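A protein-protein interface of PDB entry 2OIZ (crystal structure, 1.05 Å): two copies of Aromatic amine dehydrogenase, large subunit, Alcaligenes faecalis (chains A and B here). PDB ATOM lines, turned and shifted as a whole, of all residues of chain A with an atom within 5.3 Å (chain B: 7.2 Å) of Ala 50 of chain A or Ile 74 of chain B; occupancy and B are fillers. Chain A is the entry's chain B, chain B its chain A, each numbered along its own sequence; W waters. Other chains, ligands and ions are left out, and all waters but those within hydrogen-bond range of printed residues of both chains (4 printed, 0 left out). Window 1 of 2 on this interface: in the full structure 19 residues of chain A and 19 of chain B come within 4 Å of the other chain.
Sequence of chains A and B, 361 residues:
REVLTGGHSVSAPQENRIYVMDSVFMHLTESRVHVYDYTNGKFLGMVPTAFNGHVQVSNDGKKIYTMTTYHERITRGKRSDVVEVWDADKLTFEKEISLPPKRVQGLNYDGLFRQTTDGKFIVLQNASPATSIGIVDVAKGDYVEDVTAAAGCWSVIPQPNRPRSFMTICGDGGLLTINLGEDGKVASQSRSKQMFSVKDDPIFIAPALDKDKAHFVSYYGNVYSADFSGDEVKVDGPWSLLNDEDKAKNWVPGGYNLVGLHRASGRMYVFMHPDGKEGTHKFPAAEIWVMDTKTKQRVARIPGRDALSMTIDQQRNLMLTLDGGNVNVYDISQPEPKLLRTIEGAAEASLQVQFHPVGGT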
ATOM      1  N   LEU A  28      -1.691 -22.624 -11.846  1.00  0.00           N
ATOM      2  CA  LEU A  28      -0.599 -23.579 -12.010  1.00  0.00           C
ATOM      3  C   LEU A  28       0.748 -23.035 -11.628  1.00  0.00           C
ATOM      4  O   LEU A  28       1.700 -23.814 -11.450  1.00  0.00           O
ATOM      5  CB  LEU A  28      -0.629 -24.089 -13.467  1.00  0.00           C
ATOM      6  CG  LEU A  28       0.316 -25.206 -13.890  1.00  0.00           C
ATOM      7  CD1 LEU A  28       0.186 -26.454 -13.023  1.00  0.00           C
ATOM      8  CD2 LEU A  28       0.064 -25.545 -15.362  1.00  0.00           C
ATOM      9  N   THR A  29       0.891 -21.698 -11.519  1.00  0.00           N
ATOM     10  CA  THR A  29       2.126 -21.116 -11.012  1.00  0.00           C
ATOM     11  C   THR A  29       2.313 -21.286  -9.503  1.00  0.00           C
ATOM     12  O   THR A  29       3.370 -20.929  -9.014  1.00  0.00           O
ATOM     13  CB  THR A  29       2.289 -19.622 -11.357  1.00  0.00           C
ATOM     14  OG1 THR A  29       1.291 -18.878 -10.664  1.00  0.00           O
ATOM     15  CG2 THR A  29       2.283 -19.376 -12.854  1.00  0.00           C
ATOM     16  N   GLU A  30       1.314 -21.837  -8.794  1.00  0.00           N
ATOM     17  CA  GLU A  30       1.391 -22.066  -7.343  1.00  0.00           C
ATOM     18  C   GLU A  30       1.115 -23.525  -7.002  1.00  0.00           C
ATOM     19  O   GLU A  30       0.517 -23.845  -5.996  1.00  0.00           O
ATOM     20  CB  GLU A  30       0.517 -21.072  -6.578  1.00  0.00           C
ATOM     21  CG  GLU A  30       1.076 -20.865  -5.158  1.00  0.00           C
ATOM     22  CD  GLU A  30       0.126 -20.128  -4.245  1.00  0.00           C
ATOM     23  OE1 GLU A  30       0.133 -18.884  -4.203  1.00  0.00           O
ATOM     24  OE2 GLU A  30      -0.658 -20.824  -3.541  1.00  0.00           O
ATOM     25  N   SER A  31       1.632 -24.415  -7.843  1.00  0.00           N
ATOM     26  CA  SER A  31       1.610 -25.824  -7.552  1.00  0.00           C
ATOM     27  C   SER A  31       2.410 -26.089  -6.273  1.00  0.00           C
ATOM     28  O   SER A  31       3.271 -25.295  -5.873  1.00  0.00           O
ATOM     29  CB  SER A  31       2.188 -26.645  -8.728  1.00  0.00           C
ATOM     30  OG  SER A  31       3.603 -26.500  -8.868  1.00  0.00           O
ATOM     31  N   PRO A  48       6.436 -25.723  -1.664  1.00  0.00           N
ATOM     32  CA  PRO A  48       5.998 -24.953  -2.829  1.00  0.00           C
ATOM     33  C   PRO A  48       6.800 -25.359  -4.056  1.00  0.00           C
ATOM     34  O   PRO A  48       8.032 -25.531  -3.962  1.00  0.00           O
ATOM     35  CB  PRO A  48       6.323 -23.512  -2.408  1.00  0.00           C
ATOM     36  CG  PRO A  48       7.517 -23.635  -1.481  1.00  0.00           C
ATOM     37  CD  PRO A  48       7.198 -24.898  -0.691  1.00  0.00           C
ATOM     38  N   THR A  49       6.145 -25.450  -5.212  1.00  0.00           N
ATOM     39  CA  THR A  49       6.802 -25.889  -6.443  1.00  0.00           C
ATOM     40  C   THR A  49       6.476 -25.061  -7.664  1.00  0.00           C
ATOM     41  O   THR A  49       6.590 -25.567  -8.784  1.00  0.00           O
ATOM     42  CB  THR A  49       6.566 -27.401  -6.713  1.00  0.00           C
ATOM     43  OG1 THR A  49       5.162 -27.659  -6.831  1.00  0.00           O
ATOM     44  CG2 THR A  49       7.075 -28.292  -5.610  1.00  0.00           C
ATOM     45  N   ALA A  50       6.132 -23.795  -7.462  1.00  0.00           N
ATOM     46  CA  ALA A  50       6.057 -22.835  -8.574  1.00  0.00           C
ATOM     47  C   ALA A  50       5.231 -23.379  -9.740  1.00  0.00           C
ATOM     48  O   ALA A  50       4.138 -23.928  -9.516  1.00  0.00           O
ATOM     49  CB  ALA A  50       7.458 -22.357  -8.954  1.00  0.00           C
ATOM     50  N   PHE A  51       5.685 -23.203 -10.981  1.00  0.00           N
ATOM     51  CA  PHE A  51       4.868 -23.579 -12.127  1.00  0.00           C
ATOM     52  C   PHE A  51       4.995 -25.063 -12.422  1.00  0.00           C
ATOM     53  O   PHE A  51       6.069 -25.546 -12.772  1.00  0.00           O
ATOM     54  CB  PHE A  51       5.274 -22.779 -13.360  1.00  0.00           C
ATOM     55  CG  PHE A  51       4.471 -23.123 -14.590  1.00  0.00           C
ATOM     56  CD1 PHE A  51       3.178 -22.631 -14.750  1.00  0.00           C
ATOM     57  CD2 PHE A  51       4.986 -23.951 -15.569  1.00  0.00           C
ATOM     58  CE1 PHE A  51       2.436 -22.941 -15.877  1.00  0.00           C
ATOM     59  CE2 PHE A  51       4.235 -24.267 -16.696  1.00  0.00           C
ATOM     60  CZ  PHE A  51       2.963 -23.741 -16.868  1.00  0.00           C
ATOM     61  N   ASN A  52       3.873 -25.786 -12.321  1.00  0.00           N
ATOM     62  CA  ASN A  52       3.810 -27.196 -12.736  1.00  0.00           C
ATOM     63  C   ASN A  52       4.957 -28.014 -12.163  1.00  0.00           C
ATOM     64  O   ASN A  52       5.737 -28.660 -12.867  1.00  0.00           O
ATOM     65  CB  ASN A  52       3.811 -27.287 -14.262  1.00  0.00           C
ATOM     66  CG  ASN A  52       3.739 -28.717 -14.773  1.00  0.00           C
ATOM     67  OD1 ASN A  52       2.932 -29.569 -14.255  1.00  0.00           O
ATOM     68  ND2 ASN A  52       4.509 -29.008 -15.757  1.00  0.00           N
ATOM     69  N   GLY A  53       5.041 -28.040 -10.854  1.00  0.00           N
ATOM     70  CA  GLY A  53       6.078 -28.822 -10.200  1.00  0.00           C
ATOM     71  C   GLY A  53       5.893 -30.316 -10.410  1.00  0.00           C
ATOM     72  O   GLY A  53       4.758 -30.804 -10.552  1.00  0.00           O
ATOM     73  N   THR A  68      10.931 -27.786 -11.299  1.00  0.00           N
ATOM     74  CA  THR A  68      10.011 -26.717 -11.579  1.00  0.00           C
ATOM     75  C   THR A  68      10.640 -25.717 -12.550  1.00  0.00           C
ATOM     76  O   THR A  68      11.792 -25.861 -12.970  1.00  0.00           O
ATOM     77  CB  THR A  68       9.488 -26.060 -10.302  1.00  0.00           C
ATOM     78  OG1 THR A  68       8.411 -25.194 -10.679  1.00  0.00           O
ATOM     79  CG2 THR A  68      10.548 -25.307  -9.516  1.00  0.00           C
ATOM     80  N   THR A  69       9.823 -24.735 -12.936  1.00  0.00           N
ATOM     81  CA  THR A  69      10.221 -23.621 -13.788  1.00  0.00           C
ATOM     82  C   THR A  69       9.886 -22.315 -13.077  1.00  0.00           C
ATOM     83  O   THR A  69       8.743 -22.114 -12.631  1.00  0.00           O
ATOM     84  CB  THR A  69       9.478 -23.664 -15.139  1.00  0.00           C
ATOM     85  OG1 THR A  69       9.836 -24.860 -15.856  1.00  0.00           O
ATOM     86  CG2 THR A  69       9.731 -22.448 -16.001  1.00  0.00           C
ATOM     87  N   TYR A  70      10.861 -21.398 -13.089  1.00  0.00           N
ATOM     88  CA  TYR A  70      10.709 -20.016 -12.675  1.00  0.00           C
ATOM     89  C   TYR A  70      10.931 -19.105 -13.874  1.00  0.00           C
ATOM     90  O   TYR A  70      11.642 -19.464 -14.813  1.00  0.00           O
ATOM     91  CB  TYR A  70      11.757 -19.658 -11.606  1.00  0.00           C
ATOM     92  CG  TYR A  70      11.661 -20.452 -10.337  1.00  0.00           C
ATOM     93  CD1 TYR A  70      12.429 -21.581 -10.146  1.00  0.00           C
ATOM     94  CD2 TYR A  70      10.798 -20.081  -9.325  1.00  0.00           C
ATOM     95  CE1 TYR A  70      12.385 -22.282  -8.957  1.00  0.00           C
ATOM     96  CE2 TYR A  70      10.740 -20.786  -8.153  1.00  0.00           C
ATOM     97  CZ  TYR A  70      11.537 -21.891  -7.967  1.00  0.00           C
ATOM     98  OH  TYR A  70      11.484 -22.585  -6.739  1.00  0.00           O
ATOM     99  N   THR B  29      -0.085 -15.816  -4.657  1.00  0.00           N
ATOM    100  CA  THR B  29       0.987 -15.517  -5.610  1.00  0.00           C
ATOM    101  C   THR B  29       0.511 -15.450  -7.052  1.00  0.00           C
ATOM    102  O   THR B  29       1.305 -15.096  -7.913  1.00  0.00           O
ATOM    103  CB  THR B  29       2.160 -16.482  -5.533  1.00  0.00           C
ATOM    104  OG1 THR B  29       1.774 -17.799  -5.945  1.00  0.00           O
ATOM    105  CG2 THR B  29       2.814 -16.501  -4.138  1.00  0.00           C
ATOM    106  N   PHE B  51       2.026 -11.633  -6.522  1.00  0.00           N
ATOM    107  CA  PHE B  51       1.608 -11.754  -5.132  1.00  0.00           C
ATOM    108  C   PHE B  51       0.819 -10.509  -4.709  1.00  0.00           C
ATOM    109  O   PHE B  51       1.344  -9.404  -4.660  1.00  0.00           O
ATOM    110  CB  PHE B  51       2.826 -11.922  -4.205  1.00  0.00           C
ATOM    111  CG  PHE B  51       2.436 -12.026  -2.757  1.00  0.00           C
ATOM    112  CD1 PHE B  51       1.897 -13.201  -2.268  1.00  0.00           C
ATOM    113  CD2 PHE B  51       2.544 -10.958  -1.888  1.00  0.00           C
ATOM    114  CE1 PHE B  51       1.543 -13.318  -0.912  1.00  0.00           C
ATOM    115  CE2 PHE B  51       2.190 -11.094  -0.525  1.00  0.00           C
ATOM    116  CZ  PHE B  51       1.685 -12.278  -0.073  1.00  0.00           C
ATOM    117  N   THR B  69       4.520  -7.510  -5.819  1.00  0.00           N
ATOM    118  CA  THR B  69       5.807  -7.959  -5.280  1.00  0.00           C
ATOM    119  C   THR B  69       6.214  -9.244  -5.989  1.00  0.00           C
ATOM    120  O   THR B  69       5.411 -10.186  -6.080  1.00  0.00           O
ATOM    121  CB  THR B  69       5.695  -8.225  -3.774  1.00  0.00           C
ATOM    122  OG1 THR B  69       5.389  -7.016  -3.081  1.00  0.00           O
ATOM    123  CG2 THR B  69       6.952  -8.872  -3.196  1.00  0.00           C
ATOM    124  N   TYR B  70       7.477  -9.291  -6.410  1.00  0.00           N
ATOM    125  CA  TYR B  70       8.157 -10.489  -6.929  1.00  0.00           C
ATOM    126  C   TYR B  70       9.296 -10.861  -6.000  1.00  0.00           C
ATOM    127  O   TYR B  70       9.838 -10.013  -5.284  1.00  0.00           O
ATOM    128  CB  TYR B  70       8.759 -10.200  -8.319  1.00  0.00           C
ATOM    129  CG  TYR B  70       7.758  -9.835  -9.370  1.00  0.00           C
ATOM    130  CD1 TYR B  70       7.507  -8.498  -9.686  1.00  0.00           C
ATOM    131  CD2 TYR B  70       7.102 -10.820 -10.089  1.00  0.00           C
ATOM    132  CE1 TYR B  70       6.617  -8.163 -10.690  1.00  0.00           C
ATOM    133  CE2 TYR B  70       6.194 -10.470 -11.100  1.00  0.00           C
ATOM    134  CZ  TYR B  70       5.971  -9.126 -11.393  1.00  0.00           C
ATOM    135  OH  TYR B  70       5.102  -8.805 -12.429  1.00  0.00           O
ATOM    136  N   HIS B  71       9.659 -12.146  -6.028  1.00  0.00           N
ATOM    137  CA  HIS B  71      10.969 -12.585  -5.517  1.00  0.00           C
ATOM    138  C   HIS B  71      11.608 -13.472  -6.583  1.00  0.00           C
ATOM    139  O   HIS B  71      10.926 -14.145  -7.346  1.00  0.00           O
ATOM    140  CB  HIS B  71      10.883 -13.359  -4.195  1.00  0.00           C
ATOM    141  CG  HIS B  71      10.282 -12.584  -3.061  1.00  0.00           C
ATOM    142  ND1 HIS B  71      10.984 -11.966  -2.035  1.00  0.00           N
ATOM    143  CD2 HIS B  71       8.982 -12.324  -2.828  1.00  0.00           C
ATOM    144  CE1 HIS B  71      10.125 -11.366  -1.224  1.00  0.00           C
ATOM    145  NE2 HIS B  71       8.904 -11.591  -1.678  1.00  0.00           N
ATOM    146  N   GLU B  72      12.939 -13.528  -6.571  1.00  0.00           N
ATOM    147  CA  GLU B  72      13.643 -14.282  -7.590  1.00  0.00           C
ATOM    148  C   GLU B  72      13.179 -15.733  -7.696  1.00  0.00           C
ATOM    149  O   GLU B  72      13.184 -16.323  -8.781  1.00  0.00           O
ATOM    150  CB  GLU B  72      15.139 -14.266  -7.316  1.00  0.00           C
ATOM    151  CG  GLU B  72      15.824 -12.952  -7.375  1.00  0.00           C
ATOM    152  CD  GLU B  72      17.293 -13.063  -6.929  1.00  0.00           C
ATOM    153  OE1 GLU B  72      17.617 -13.426  -5.729  1.00  0.00           O
ATOM    154  OE2 GLU B  72      18.150 -12.753  -7.783  1.00  0.00           O
ATOM    155  N   ARG B  73      12.869 -16.353  -6.553  1.00  0.00           N
ATOM    156  CA  ARG B  73      12.372 -17.707  -6.501  1.00  0.00           C
ATOM    157  C   ARG B  73      11.064 -17.792  -5.714  1.00  0.00           C
ATOM    158  O   ARG B  73      10.775 -18.820  -5.124  1.00  0.00           O
ATOM    159  CB  ARG B  73      13.450 -18.629  -5.986  1.00  0.00           C
ATOM    160  CG  ARG B  73      14.672 -18.728  -6.863  1.00  0.00           C
ATOM    161  CD  ARG B  73      14.424 -19.603  -8.045  1.00  0.00           C
ATOM    162  NE  ARG B  73      15.627 -19.845  -8.834  1.00  0.00           N
ATOM    163  CZ  ARG B  73      16.096 -19.059  -9.774  1.00  0.00           C
ATOM    164  NH1 ARG B  73      15.438 -17.995 -10.157  1.00  0.00           N
ATOM    165  NH2 ARG B  73      17.236 -19.388 -10.370  1.00  0.00           N
ATOM    166  N   ILE B  74      10.275 -16.712  -5.760  1.00  0.00           N
ATOM    167  CA  ILE B  74       8.920 -16.610  -5.217  1.00  0.00           C
ATOM    168  C   ILE B  74       8.882 -16.609  -3.705  1.00  0.00           C
ATOM    169  O   ILE B  74       8.547 -15.594  -3.098  1.00  0.00           O
ATOM    170  CB  ILE B  74       7.936 -17.682  -5.819  1.00  0.00           C
ATOM    171  CG1 ILE B  74       7.999 -17.703  -7.348  1.00  0.00           C
ATOM    172  CG2 ILE B  74       6.522 -17.376  -5.301  1.00  0.00           C
ATOM    173  CD1 ILE B  74       7.335 -18.882  -7.945  1.00  0.00           C
ATOM    174  N   THR B  75       9.261 -17.744  -3.110  1.00  0.00           N
ATOM    175  CA  THR B  75       9.279 -17.928  -1.663  1.00  0.00           C
ATOM    176  C   THR B  75      10.690 -17.778  -1.073  1.00  0.00           C
ATOM    177  O   THR B  75      10.862 -17.901   0.137  1.00  0.00           O
ATOM    178  CB  THR B  75       8.693 -19.309  -1.316  1.00  0.00           C
ATOM    179  OG1 THR B  75       9.254 -20.309  -2.184  1.00  0.00           O
ATOM    180  CG2 THR B  75       7.203 -19.314  -1.491  1.00  0.00           C
ATOM    181  N   ARG B  76      11.675 -17.472  -1.930  1.00  0.00           N
ATOM    182  CA  ARG B  76      13.037 -17.134  -1.475  1.00  0.00           C
ATOM    183  C   ARG B  76      13.648 -16.245  -2.540  1.00  0.00           C
ATOM    184  O   ARG B  76      13.084 -16.059  -3.624  1.00  0.00           O
ATOM    185  CB  ARG B  76      13.882 -18.383  -1.264  1.00  0.00           C
ATOM    186  CG  ARG B  76      14.068 -19.232  -2.503  1.00  0.00           C
ATOM    187  CD  ARG B  76      14.774 -20.574  -2.228  1.00  0.00           C
ATOM    188  NE  ARG B  76      14.754 -21.405  -3.415  1.00  0.00           N
ATOM    189  CZ  ARG B  76      15.641 -21.319  -4.399  1.00  0.00           C
ATOM    190  NH1 ARG B  76      16.703 -20.525  -4.270  1.00  0.00           N
ATOM    191  NH2 ARG B  76      15.497 -22.054  -5.502  1.00  0.00           N
ATOM    192  N   GLY B  77      14.789 -15.659  -2.202  1.00  0.00           N
ATOM    193  CA  GLY B  77      15.464 -14.763  -3.126  1.00  0.00           C
ATOM    194  C   GLY B  77      15.061 -13.312  -2.935  1.00  0.00           C
ATOM    195  O   GLY B  77      14.202 -12.950  -2.122  1.00  0.00           O
ATOM    196  N   LYS B  78      15.712 -12.455  -3.712  1.00  0.00           N
ATOM    197  CA  LYS B  78      15.568 -11.017  -3.563  1.00  0.00           C
ATOM    198  C   LYS B  78      14.158 -10.563  -3.929  1.00  0.00           C
ATOM    199  O   LYS B  78      13.595 -10.981  -4.953  1.00  0.00           O
ATOM    200  CB  LYS B  78      16.583 -10.281  -4.438  1.00  0.00           C
ATOM    201  CG  LYS B  78      16.550  -8.754  -4.244  1.00  0.00           C
ATOM    202  CD  LYS B  78      17.718  -8.008  -4.874  1.00  0.00           C
ATOM    203  CE  LYS B  78      17.744  -6.547  -4.375  1.00  0.00           C
ATOM    204  NZ  LYS B  78      18.992  -5.820  -4.729  1.00  0.00           N
HETATM  205  O   HOH W   1      12.222 -22.870  -3.576  1.00  0.00           O
HETATM  206  O   HOH W   2       3.906 -19.245  -6.907  1.00  0.00           O
HETATM  207  O   HOH W   3       2.092 -16.258 -10.266  1.00  0.00           O
HETATM  208  O   HOH W   4      10.460 -21.451  -4.763  1.00  0.00           O
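Of the printed residues of chain B, Glu 30 of chain A touches Thr 29 (2.6 Å). Printed residues of chain B within 4 Å of Tyr 70 of chain A: Arg 73 and Ile 74. Of the printed residues of chain A, Thr 29 of chain B touches Glu 30 (2.6 Å). His 71 of chain B touches none of the printed residues of chain A. Ile 74 of chain B touches two residues of chain A. Of the printed residues of chain A, Thr 75 of chain B touches Pro 48 (3.8 Å). The nearest residue of chain A that does not touch Ile 74 of chain B is Thr 29 of chain A (4.6 Å).
Among the printed residues, merely in contact across the chains: Tyr 70 of chain A with Arg 73 of chain B (3.5 Å), Ala 50 of chain A with Ile 74 of chain B (3.6 Å), Pro 48 of chain A with Thr 75 of chain B (3.8 Å) and Tyr 70 of chain A with Ile 74 of chain B (3.9 Å).
OG1 of Thr 29 of chain B is in hydrogen-bond range of OE1 of Glu 30 of chain A (2.6 Å).
Water W4 lies within hydrogen-bond range of the side-chain hydroxyl (OH) of Tyr 70 of chain A (2.5 Å), the backbone carbonyl oxygen (O) of Arg 73 of chain B (2.7 Å) and the side-chain hydroxyl (OG1) of Thr 75 of chain B (3.1 Å). Water W3 lies within hydrogen-bond range of the backbone carbonyl oxygen (O) of Thr 29 of chain B (2.7 Å) and the side-chain hydroxyl (OG1) of Thr 29 of chain A (2.8 Å). Water W2 bridges the backbone carbonyl oxygen (O) of Thr 29 of chain A (2.8 Å) and the side-chain hydroxyl (OG1) of Thr 29 of chain B (2.7 Å). Water W1 bridges the guanidinium group of Arg 76 of chain B (2.9 Å) and the side-chain hydroxyl of Tyr 70 of chain A (3.3 Å).
Positions printed for both chains: 29, 51, 69 and 70. Of the 5 pairs that touch across the chains among the printed residues, none has its exchanged pair printed and touching as well.
The side-chain hydroxyl of Ser 31 of chain A is in hydrogen-bond range of the backbone carbonyl oxygen of Ala 50 of chain A, at 2.7 Å.
Hydrophobic or aromatic side chains of chain B within 4 Å of the printed part of chain A: Ile 74. Along chain A the printed residues that touch a printed residue of chain B span positions 30 to 70. Among the printed residues, no Asp or Glu carboxylate lies within 4 Å of a Lys or Arg side-chain nitrogen of the other chain.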
